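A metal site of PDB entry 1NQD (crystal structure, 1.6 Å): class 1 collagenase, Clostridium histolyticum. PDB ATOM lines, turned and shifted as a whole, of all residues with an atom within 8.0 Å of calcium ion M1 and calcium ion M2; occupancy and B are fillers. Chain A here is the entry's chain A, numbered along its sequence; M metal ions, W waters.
The side-chain amide oxygen (OD1) of Asn 16 lies within hydrogen-bond range of the backbone NH (N) of Asp 18 (2.8 Å). The side-chain hydroxyl (OH) of Tyr 116 sits close to the side-chain carboxylate (OD2) of Asp 44 (2.5 Å). O of Val 107 sits at hydrogen-bond distance from N of Asp 44, 2.8 Å away. The side-chain carboxylate (OE1) of Glu 13 lies close to the side-chain amide nitrogen (ND2) of Asn 17. O of Asn 17 lies within hydrogen-bond range of N of Tyr 45 (2.8 Å). ND2 of Asn 17 lies within hydrogen-bond range of OG1 of Thr 24 (3.4 Å). The backbone NH (N) of Glu 13 lies within hydrogen-bond range of the backbone carbonyl oxygen (O) of Gln 34 (2.9 Å).
Six residues have an atom within 4 Å of calcium ion M1: Glu 15, Asn 17, Asp 18, Asp 41, Arg 43 and Asp 44.
Of the 25 residues printed, 5 come within 4 Å of calcium ion M2.
Calcium ion M1 is bound by the side-chain carboxylate (OD2) of Asp 18 (2.3 Å), the backbone carbonyl oxygen (O) of Arg 43 (2.3 Å), the side-chain carboxylate (OD1) of Asp 44 (2.3 Å), the side-chain amide oxygen (OD1) of Asn 17 (2.4 Å), the side-chain carboxylate (OD1) of Asp 41 (2.4 Å), the side-chain carboxylate (OE2) of Glu 15 (2.5 Å) and the side-chain carboxylate (OE1) of Glu 15 (2.6 Å). Calcium ion M1 has seven donor atoms within binding distance.
Calcium ion M2 is bound by OE2 of Glu 15 (2.2 Å). OD2 of Asp 41 binds calcium ion M2 (2.3 Å). Calcium ion M2 is bound by the backbone carbonyl oxygen (O) of Ser 36 (2.4 Å). Calcium ion M2 is bound by OE1 of Glu 13 (2.5 Å). The side-chain carboxylate (OD1) of Asp 44 binds calcium ion M2 (2.5 Å). Calcium ion M2 is bound by water W1 (2.5 Å). OE2 of Glu 13 binds calcium ion M2 (2.5 Å). Calcium ion M2 is bound by OD2 of Asp 44.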
ATOM      1  N   GLU A  13      -1.202 -19.992  25.641  1.00  0.00           N
ATOM      2  CA  GLU A  13      -1.389 -21.250  24.902  1.00  0.00           C
ATOM      3  C   GLU A  13      -0.179 -21.547  24.051  1.00  0.00           C
ATOM      4  O   GLU A  13       0.656 -20.663  23.826  1.00  0.00           O
ATOM      5  CB  GLU A  13      -2.667 -21.144  24.041  1.00  0.00           C
ATOM      6  CG  GLU A  13      -2.519 -20.079  22.966  1.00  0.00           C
ATOM      7  CD  GLU A  13      -3.654 -20.137  21.940  1.00  0.00           C
ATOM      8  OE1 GLU A  13      -3.861 -21.217  21.352  1.00  0.00           O
ATOM      9  OE2 GLU A  13      -4.021 -19.034  21.463  1.00  0.00           O
ATOM     10  N   LYS A  14      -0.023 -22.767  23.534  1.00  0.00           N
ATOM     11  CA  LYS A  14       1.073 -23.070  22.608  1.00  0.00           C
ATOM     12  C   LYS A  14       0.526 -23.724  21.345  1.00  0.00           C
ATOM     13  O   LYS A  14       0.128 -24.884  21.308  1.00  0.00           O
ATOM     14  CB  LYS A  14       2.142 -23.929  23.279  1.00  0.00           C
ATOM     15  CG  LYS A  14       2.634 -23.430  24.629  1.00  0.00           C
ATOM     16  CD  LYS A  14       3.688 -22.340  24.526  1.00  0.00           C
ATOM     17  CE  LYS A  14       3.147 -20.993  24.998  1.00  0.00           C
ATOM     18  NZ  LYS A  14       4.241 -20.124  25.534  1.00  0.00           N
ATOM     19  N   GLU A  15       0.451 -22.958  20.240  1.00  0.00           N
ATOM     20  CA  GLU A  15       0.021 -23.575  18.999  1.00  0.00           C
ATOM     21  C   GLU A  15       1.144 -24.469  18.426  1.00  0.00           C
ATOM     22  O   GLU A  15       2.294 -24.157  18.760  1.00  0.00           O
ATOM     23  CB  GLU A  15      -0.331 -22.530  17.927  1.00  0.00           C
ATOM     24  CG  GLU A  15      -1.517 -21.642  18.293  1.00  0.00           C
ATOM     25  CD  GLU A  15      -2.857 -22.304  18.041  1.00  0.00           C
ATOM     26  OE1 GLU A  15      -2.927 -23.416  17.491  1.00  0.00           O
ATOM     27  OE2 GLU A  15      -3.876 -21.693  18.453  1.00  0.00           O
ATOM     28  N   ASN A  16       0.818 -25.462  17.628  1.00  0.00           N
ATOM     29  CA  ASN A  16      -0.500 -25.862  17.209  1.00  0.00           C
ATOM     30  C   ASN A  16      -1.180 -26.712  18.285  1.00  0.00           C
ATOM     31  O   ASN A  16      -0.577 -27.679  18.767  1.00  0.00           O
ATOM     32  CB  ASN A  16      -0.467 -26.679  15.906  1.00  0.00           C
ATOM     33  CG  ASN A  16      -1.853 -26.996  15.401  1.00  0.00           C
ATOM     34  OD1 ASN A  16      -2.580 -27.851  15.922  1.00  0.00           O
ATOM     35  ND2 ASN A  16      -2.262 -26.288  14.346  1.00  0.00           N
ATOM     36  N   ASN A  17      -2.390 -26.329  18.653  1.00  0.00           N
ATOM     37  CA  ASN A  17      -3.105 -27.144  19.644  1.00  0.00           C
ATOM     38  C   ASN A  17      -4.478 -27.501  19.120  1.00  0.00           C
ATOM     39  O   ASN A  17      -5.477 -27.511  19.839  1.00  0.00           O
ATOM     40  CB  ASN A  17      -3.205 -26.359  20.959  1.00  0.00           C
ATOM     41  CG  ASN A  17      -3.774 -24.962  20.756  1.00  0.00           C
ATOM     42  OD1 ASN A  17      -4.395 -24.680  19.725  1.00  0.00           O
ATOM     43  ND2 ASN A  17      -3.581 -24.107  21.765  1.00  0.00           N
ATOM     44  N   ASP A  18      -4.584 -27.815  17.811  1.00  0.00           N
ATOM     45  CA  ASP A  18      -5.950 -27.953  17.324  1.00  0.00           C
ATOM     46  C   ASP A  18      -6.545 -29.335  17.550  1.00  0.00           C
ATOM     47  O   ASP A  18      -7.702 -29.564  17.173  1.00  0.00           O
ATOM     48  CB  ASP A  18      -5.987 -27.544  15.836  1.00  0.00           C
ATOM     49  CG  ASP A  18      -5.412 -26.159  15.609  1.00  0.00           C
ATOM     50  OD1 ASP A  18      -4.998 -25.802  14.480  1.00  0.00           O
ATOM     51  OD2 ASP A  18      -5.359 -25.352  16.564  1.00  0.00           O
ATOM     52  N   SER A  19      -5.835 -30.279  18.173  1.00  0.00           N
ATOM     53  CA  SER A  19      -6.427 -31.587  18.436  1.00  0.00           C
ATOM     54  C   SER A  19      -5.893 -32.108  19.771  1.00  0.00           C
ATOM     55  O   SER A  19      -4.942 -31.548  20.307  1.00  0.00           O
ATOM     56  CB  SER A  19      -6.147 -32.576  17.297  1.00  0.00           C
ATOM     57  OG  SER A  19      -4.749 -32.636  17.107  1.00  0.00           O
ATOM     58  N   LYS A  22      -2.343 -32.698  20.649  1.00  0.00           N
ATOM     59  CA  LYS A  22      -1.514 -31.503  20.716  1.00  0.00           C
ATOM     60  C   LYS A  22      -1.980 -30.472  21.757  1.00  0.00           C
ATOM     61  O   LYS A  22      -1.622 -29.302  21.734  1.00  0.00           O
ATOM     62  CB  LYS A  22      -1.455 -30.834  19.338  1.00  0.00           C
ATOM     63  CG  LYS A  22      -0.737 -31.694  18.311  1.00  0.00           C
ATOM     64  CD  LYS A  22      -1.068 -31.230  16.897  1.00  0.00           C
ATOM     65  CE  LYS A  22      -0.944 -32.367  15.886  1.00  0.00           C
ATOM     66  NZ  LYS A  22       0.468 -32.574  15.460  1.00  0.00           N
ATOM     67  N   THR A  24      -2.568 -28.042  24.828  1.00  0.00           N
ATOM     68  CA  THR A  24      -1.717 -27.250  25.709  1.00  0.00           C
ATOM     69  C   THR A  24      -1.982 -27.640  27.153  1.00  0.00           C
ATOM     70  O   THR A  24      -3.165 -27.640  27.499  1.00  0.00           O
ATOM     71  CB  THR A  24      -2.047 -25.760  25.563  1.00  0.00           C
ATOM     72  OG1 THR A  24      -1.644 -25.341  24.252  1.00  0.00           O
ATOM     73  CG2 THR A  24      -1.301 -24.871  26.554  1.00  0.00           C
ATOM     74  N   GLN A  34      -3.883 -17.763  28.592  1.00  0.00           N
ATOM     75  CA  GLN A  34      -4.259 -16.745  27.615  1.00  0.00           C
ATOM     76  C   GLN A  34      -4.271 -17.344  26.205  1.00  0.00           C
ATOM     77  O   GLN A  34      -3.317 -17.983  25.785  1.00  0.00           O
ATOM     78  CB  GLN A  34      -3.308 -15.548  27.624  1.00  0.00           C
ATOM     79  CG  GLN A  34      -3.409 -14.713  28.898  1.00  0.00           C
ATOM     80  CD  GLN A  34      -2.719 -13.369  28.769  1.00  0.00           C
ATOM     81  OE1 GLN A  34      -2.767 -12.558  29.691  1.00  0.00           O
ATOM     82  NE2 GLN A  34      -2.075 -13.152  27.625  1.00  0.00           N
ATOM     83  N   GLY A  35      -5.369 -17.081  25.485  1.00  0.00           N
ATOM     84  CA  GLY A  35      -5.344 -17.581  24.118  1.00  0.00           C
ATOM     85  C   GLY A  35      -6.125 -16.677  23.168  1.00  0.00           C
ATOM     86  O   GLY A  35      -6.702 -15.665  23.536  1.00  0.00           O
ATOM     87  N   SER A  36      -6.094 -17.087  21.902  1.00  0.00           N
ATOM     88  CA  SER A  36      -6.817 -16.325  20.891  1.00  0.00           C
ATOM     89  C   SER A  36      -7.285 -17.303  19.806  1.00  0.00           C
ATOM     90  O   SER A  36      -6.670 -18.337  19.598  1.00  0.00           O
ATOM     91  CB  SER A  36      -6.010 -15.166  20.336  1.00  0.00           C
ATOM     92  OG  SER A  36      -4.951 -15.643  19.524  1.00  0.00           O
ATOM     93  N   LEU A  37      -8.352 -16.913  19.146  1.00  0.00           N
ATOM     94  CA  LEU A  37      -8.913 -17.658  18.017  1.00  0.00           C
ATOM     95  C   LEU A  37      -9.179 -16.638  16.900  1.00  0.00           C
ATOM     96  O   LEU A  37     -10.326 -16.271  16.683  1.00  0.00           O
ATOM     97  CB  LEU A  37     -10.158 -18.452  18.384  1.00  0.00           C
ATOM     98  CG  LEU A  37      -9.981 -19.516  19.489  1.00  0.00           C
ATOM     99  CD1 LEU A  37     -11.290 -19.745  20.212  1.00  0.00           C
ATOM    100  CD2 LEU A  37      -9.476 -20.825  18.870  1.00  0.00           C
ATOM    101  N   LEU A  38      -8.107 -16.255  16.224  1.00  0.00           N
ATOM    102  CA  LEU A  38      -8.124 -15.266  15.149  1.00  0.00           C
ATOM    103  C   LEU A  38      -8.200 -15.950  13.800  1.00  0.00           C
ATOM    104  O   LEU A  38      -7.495 -16.929  13.556  1.00  0.00           O
ATOM    105  CB  LEU A  38      -6.871 -14.391  15.209  1.00  0.00           C
ATOM    106  CG  LEU A  38      -6.654 -13.715  16.580  1.00  0.00           C
ATOM    107  CD1 LEU A  38      -5.354 -12.914  16.564  1.00  0.00           C
ATOM    108  CD2 LEU A  38      -7.856 -12.861  16.927  1.00  0.00           C
ATOM    109  N   ASP A  40      -8.570 -18.413  10.860  1.00  0.00           N
ATOM    110  CA  ASP A  40      -8.899 -19.823  10.729  1.00  0.00           C
ATOM    111  C   ASP A  40      -8.387 -20.648  11.905  1.00  0.00           C
ATOM    112  O   ASP A  40      -8.501 -21.869  11.831  1.00  0.00           O
ATOM    113  CB  ASP A  40      -8.375 -20.376   9.405  1.00  0.00           C
ATOM    114  CG  ASP A  40      -6.889 -20.391   9.227  1.00  0.00           C
ATOM    115  OD1 ASP A  40      -6.127 -20.376  10.213  1.00  0.00           O
ATOM    116  OD2 ASP A  40      -6.437 -20.414   8.047  1.00  0.00           O
ATOM    117  N   ASP A  41      -7.899 -19.975  12.945  1.00  0.00           N
ATOM    118  CA  ASP A  41      -7.593 -20.638  14.201  1.00  0.00           C
ATOM    119  C   ASP A  41      -8.897 -20.659  15.011  1.00  0.00           C
ATOM    120  O   ASP A  41      -9.210 -19.661  15.670  1.00  0.00           O
ATOM    121  CB  ASP A  41      -6.479 -19.962  14.982  1.00  0.00           C
ATOM    122  CG  ASP A  41      -6.151 -20.681  16.288  1.00  0.00           C
ATOM    123  OD1 ASP A  41      -6.248 -21.926  16.312  1.00  0.00           O
ATOM    124  OD2 ASP A  41      -5.819 -20.027  17.299  1.00  0.00           O
ATOM    125  N   SER A  42      -9.640 -21.758  14.916  1.00  0.00           N
ATOM    126  CA  SER A  42     -10.967 -21.846  15.486  1.00  0.00           C
ATOM    127  C   SER A  42     -11.041 -22.839  16.650  1.00  0.00           C
ATOM    128  O   SER A  42     -12.127 -22.937  17.224  1.00  0.00           O
ATOM    129  CB  SER A  42     -12.015 -22.292  14.460  1.00  0.00           C
ATOM    130  OG  SER A  42     -11.713 -23.545  13.888  1.00  0.00           O
ATOM    131  N   ARG A  43      -9.936 -23.520  16.910  1.00  0.00           N
ATOM    132  CA  ARG A  43      -9.929 -24.505  17.976  1.00  0.00           C
ATOM    133  C   ARG A  43      -8.627 -24.461  18.748  1.00  0.00           C
ATOM    134  O   ARG A  43      -7.544 -24.441  18.157  1.00  0.00           O
ATOM    135  CB  ARG A  43     -10.104 -25.942  17.424  1.00  0.00           C
ATOM    136  CG  ARG A  43     -11.270 -26.066  16.444  1.00  0.00           C
ATOM    137  CD  ARG A  43     -11.215 -27.328  15.629  1.00  0.00           C
ATOM    138  NE  ARG A  43     -10.898 -28.563  16.321  1.00  0.00           N
ATOM    139  CZ  ARG A  43     -11.742 -29.505  16.718  1.00  0.00           C
ATOM    140  NH1 ARG A  43     -13.059 -29.430  16.546  1.00  0.00           N
ATOM    141  NH2 ARG A  43     -11.236 -30.577  17.328  1.00  0.00           N
ATOM    142  N   ASP A  44      -8.758 -24.475  20.082  1.00  0.00           N
ATOM    143  CA  ASP A  44      -7.581 -24.516  20.955  1.00  0.00           C
ATOM    144  C   ASP A  44      -7.801 -25.586  22.016  1.00  0.00           C
ATOM    145  O   ASP A  44      -8.712 -25.443  22.862  1.00  0.00           O
ATOM    146  CB  ASP A  44      -7.380 -23.176  21.640  1.00  0.00           C
ATOM    147  CG  ASP A  44      -6.923 -22.031  20.765  1.00  0.00           C
ATOM    148  OD1 ASP A  44      -6.397 -22.280  19.660  1.00  0.00           O
ATOM    149  OD2 ASP A  44      -6.892 -20.906  21.286  1.00  0.00           O
ATOM    150  N   TYR A  45      -7.039 -26.664  21.987  1.00  0.00           N
ATOM    151  CA  TYR A  45      -7.202 -27.754  22.954  1.00  0.00           C
ATOM    152  C   TYR A  45      -6.278 -27.572  24.144  1.00  0.00           C
ATOM    153  O   TYR A  45      -5.104 -27.216  24.028  1.00  0.00           O
ATOM    154  CB  TYR A  45      -6.910 -29.122  22.347  1.00  0.00           C
ATOM    155  CG  TYR A  45      -8.098 -30.035  22.219  1.00  0.00           C
ATOM    156  CD1 TYR A  45      -8.568 -30.470  20.986  1.00  0.00           C
ATOM    157  CD2 TYR A  45      -8.759 -30.475  23.354  1.00  0.00           C
ATOM    158  CE1 TYR A  45      -9.662 -31.304  20.898  1.00  0.00           C
ATOM    159  CE2 TYR A  45      -9.842 -31.303  23.279  1.00  0.00           C
ATOM    160  CZ  TYR A  45     -10.299 -31.721  22.049  1.00  0.00           C
ATOM    161  OH  TYR A  45     -11.392 -32.557  22.023  1.00  0.00           O
ATOM    162  N   TYR A  46      -6.872 -27.854  25.306  1.00  0.00           N
ATOM    163  CA  TYR A  46      -6.123 -27.873  26.550  1.00  0.00           C
ATOM    164  C   TYR A  46      -6.360 -29.207  27.267  1.00  0.00           C
ATOM    165  O   TYR A  46      -7.312 -29.911  27.007  1.00  0.00           O
ATOM    166  CB  TYR A  46      -6.575 -26.746  27.479  1.00  0.00           C
ATOM    167  CG  TYR A  46      -6.355 -25.347  26.949  1.00  0.00           C
ATOM    168  CD1 TYR A  46      -7.290 -24.767  26.078  1.00  0.00           C
ATOM    169  CD2 TYR A  46      -5.229 -24.634  27.319  1.00  0.00           C
ATOM    170  CE1 TYR A  46      -7.009 -23.484  25.647  1.00  0.00           C
ATOM    171  CE2 TYR A  46      -4.945 -23.339  26.881  1.00  0.00           C
ATOM    172  CZ  TYR A  46      -5.885 -22.790  26.013  1.00  0.00           C
ATOM    173  OH  TYR A  46      -5.667 -21.521  25.557  1.00  0.00           O
ATOM    174  N   LEU A 106     -11.735 -28.478  24.957  1.00  0.00           N
ATOM    175  CA  LEU A 106     -11.700 -27.889  23.632  1.00  0.00           C
ATOM    176  C   LEU A 106     -12.328 -26.500  23.702  1.00  0.00           C
ATOM    177  O   LEU A 106     -13.542 -26.434  23.960  1.00  0.00           O
ATOM    178  CB  LEU A 106     -12.463 -28.818  22.693  1.00  0.00           C
ATOM    179  CG  LEU A 106     -12.677 -28.259  21.273  1.00  0.00           C
ATOM    180  CD1 LEU A 106     -11.323 -27.895  20.703  1.00  0.00           C
ATOM    181  CD2 LEU A 106     -13.442 -29.269  20.419  1.00  0.00           C
ATOM    182  N   VAL A 107     -11.530 -25.476  23.485  1.00  0.00           N
ATOM    183  CA  VAL A 107     -12.065 -24.119  23.346  1.00  0.00           C
ATOM    184  C   VAL A 107     -12.243 -23.891  21.845  1.00  0.00           C
ATOM    185  O   VAL A 107     -11.304 -24.110  21.086  1.00  0.00           O
ATOM    186  CB  VAL A 107     -11.142 -23.065  23.927  1.00  0.00           C
ATOM    187  CG1 VAL A 107     -11.627 -21.648  23.710  1.00  0.00           C
ATOM    188  CG2 VAL A 107     -10.960 -23.274  25.433  1.00  0.00           C
ATOM    189  N   GLY A 114     -11.390 -13.622  18.100  1.00  0.00           N
ATOM    190  CA  GLY A 114     -11.101 -12.813  19.287  1.00  0.00           C
ATOM    191  C   GLY A 114     -10.168 -13.532  20.271  1.00  0.00           C
ATOM    192  O   GLY A 114      -9.605 -14.576  19.958  1.00  0.00           O
ATOM    193  N   TYR A 116      -9.324 -14.669  24.562  1.00  0.00           N
ATOM    194  CA  TYR A 116      -9.976 -15.178  25.764  1.00  0.00           C
ATOM    195  C   TYR A 116      -8.932 -15.545  26.808  1.00  0.00           C
ATOM    196  O   TYR A 116      -7.758 -15.660  26.477  1.00  0.00           O
ATOM    197  CB  TYR A 116     -10.846 -16.419  25.471  1.00  0.00           C
ATOM    198  CG  TYR A 116      -9.964 -17.542  24.944  1.00  0.00           C
ATOM    199  CD1 TYR A 116      -9.465 -18.489  25.837  1.00  0.00           C
ATOM    200  CD2 TYR A 116      -9.614 -17.677  23.604  1.00  0.00           C
ATOM    201  CE1 TYR A 116      -8.658 -19.517  25.410  1.00  0.00           C
ATOM    202  CE2 TYR A 116      -8.799 -18.717  23.174  1.00  0.00           C
ATOM    203  CZ  TYR A 116      -8.327 -19.642  24.082  1.00  0.00           C
ATOM    204  OH  TYR A 116      -7.500 -20.680  23.684  1.00  0.00           O
HETATM  205 CA    CA M   1      -5.448 -23.538  17.959  1.00  0.00          CA
HETATM  206 CA    CA M   2      -5.122 -20.170  19.518  1.00  0.00          CA
HETATM  207  O   HOH W   1      -3.295 -18.777  18.580  1.00  0.00           O
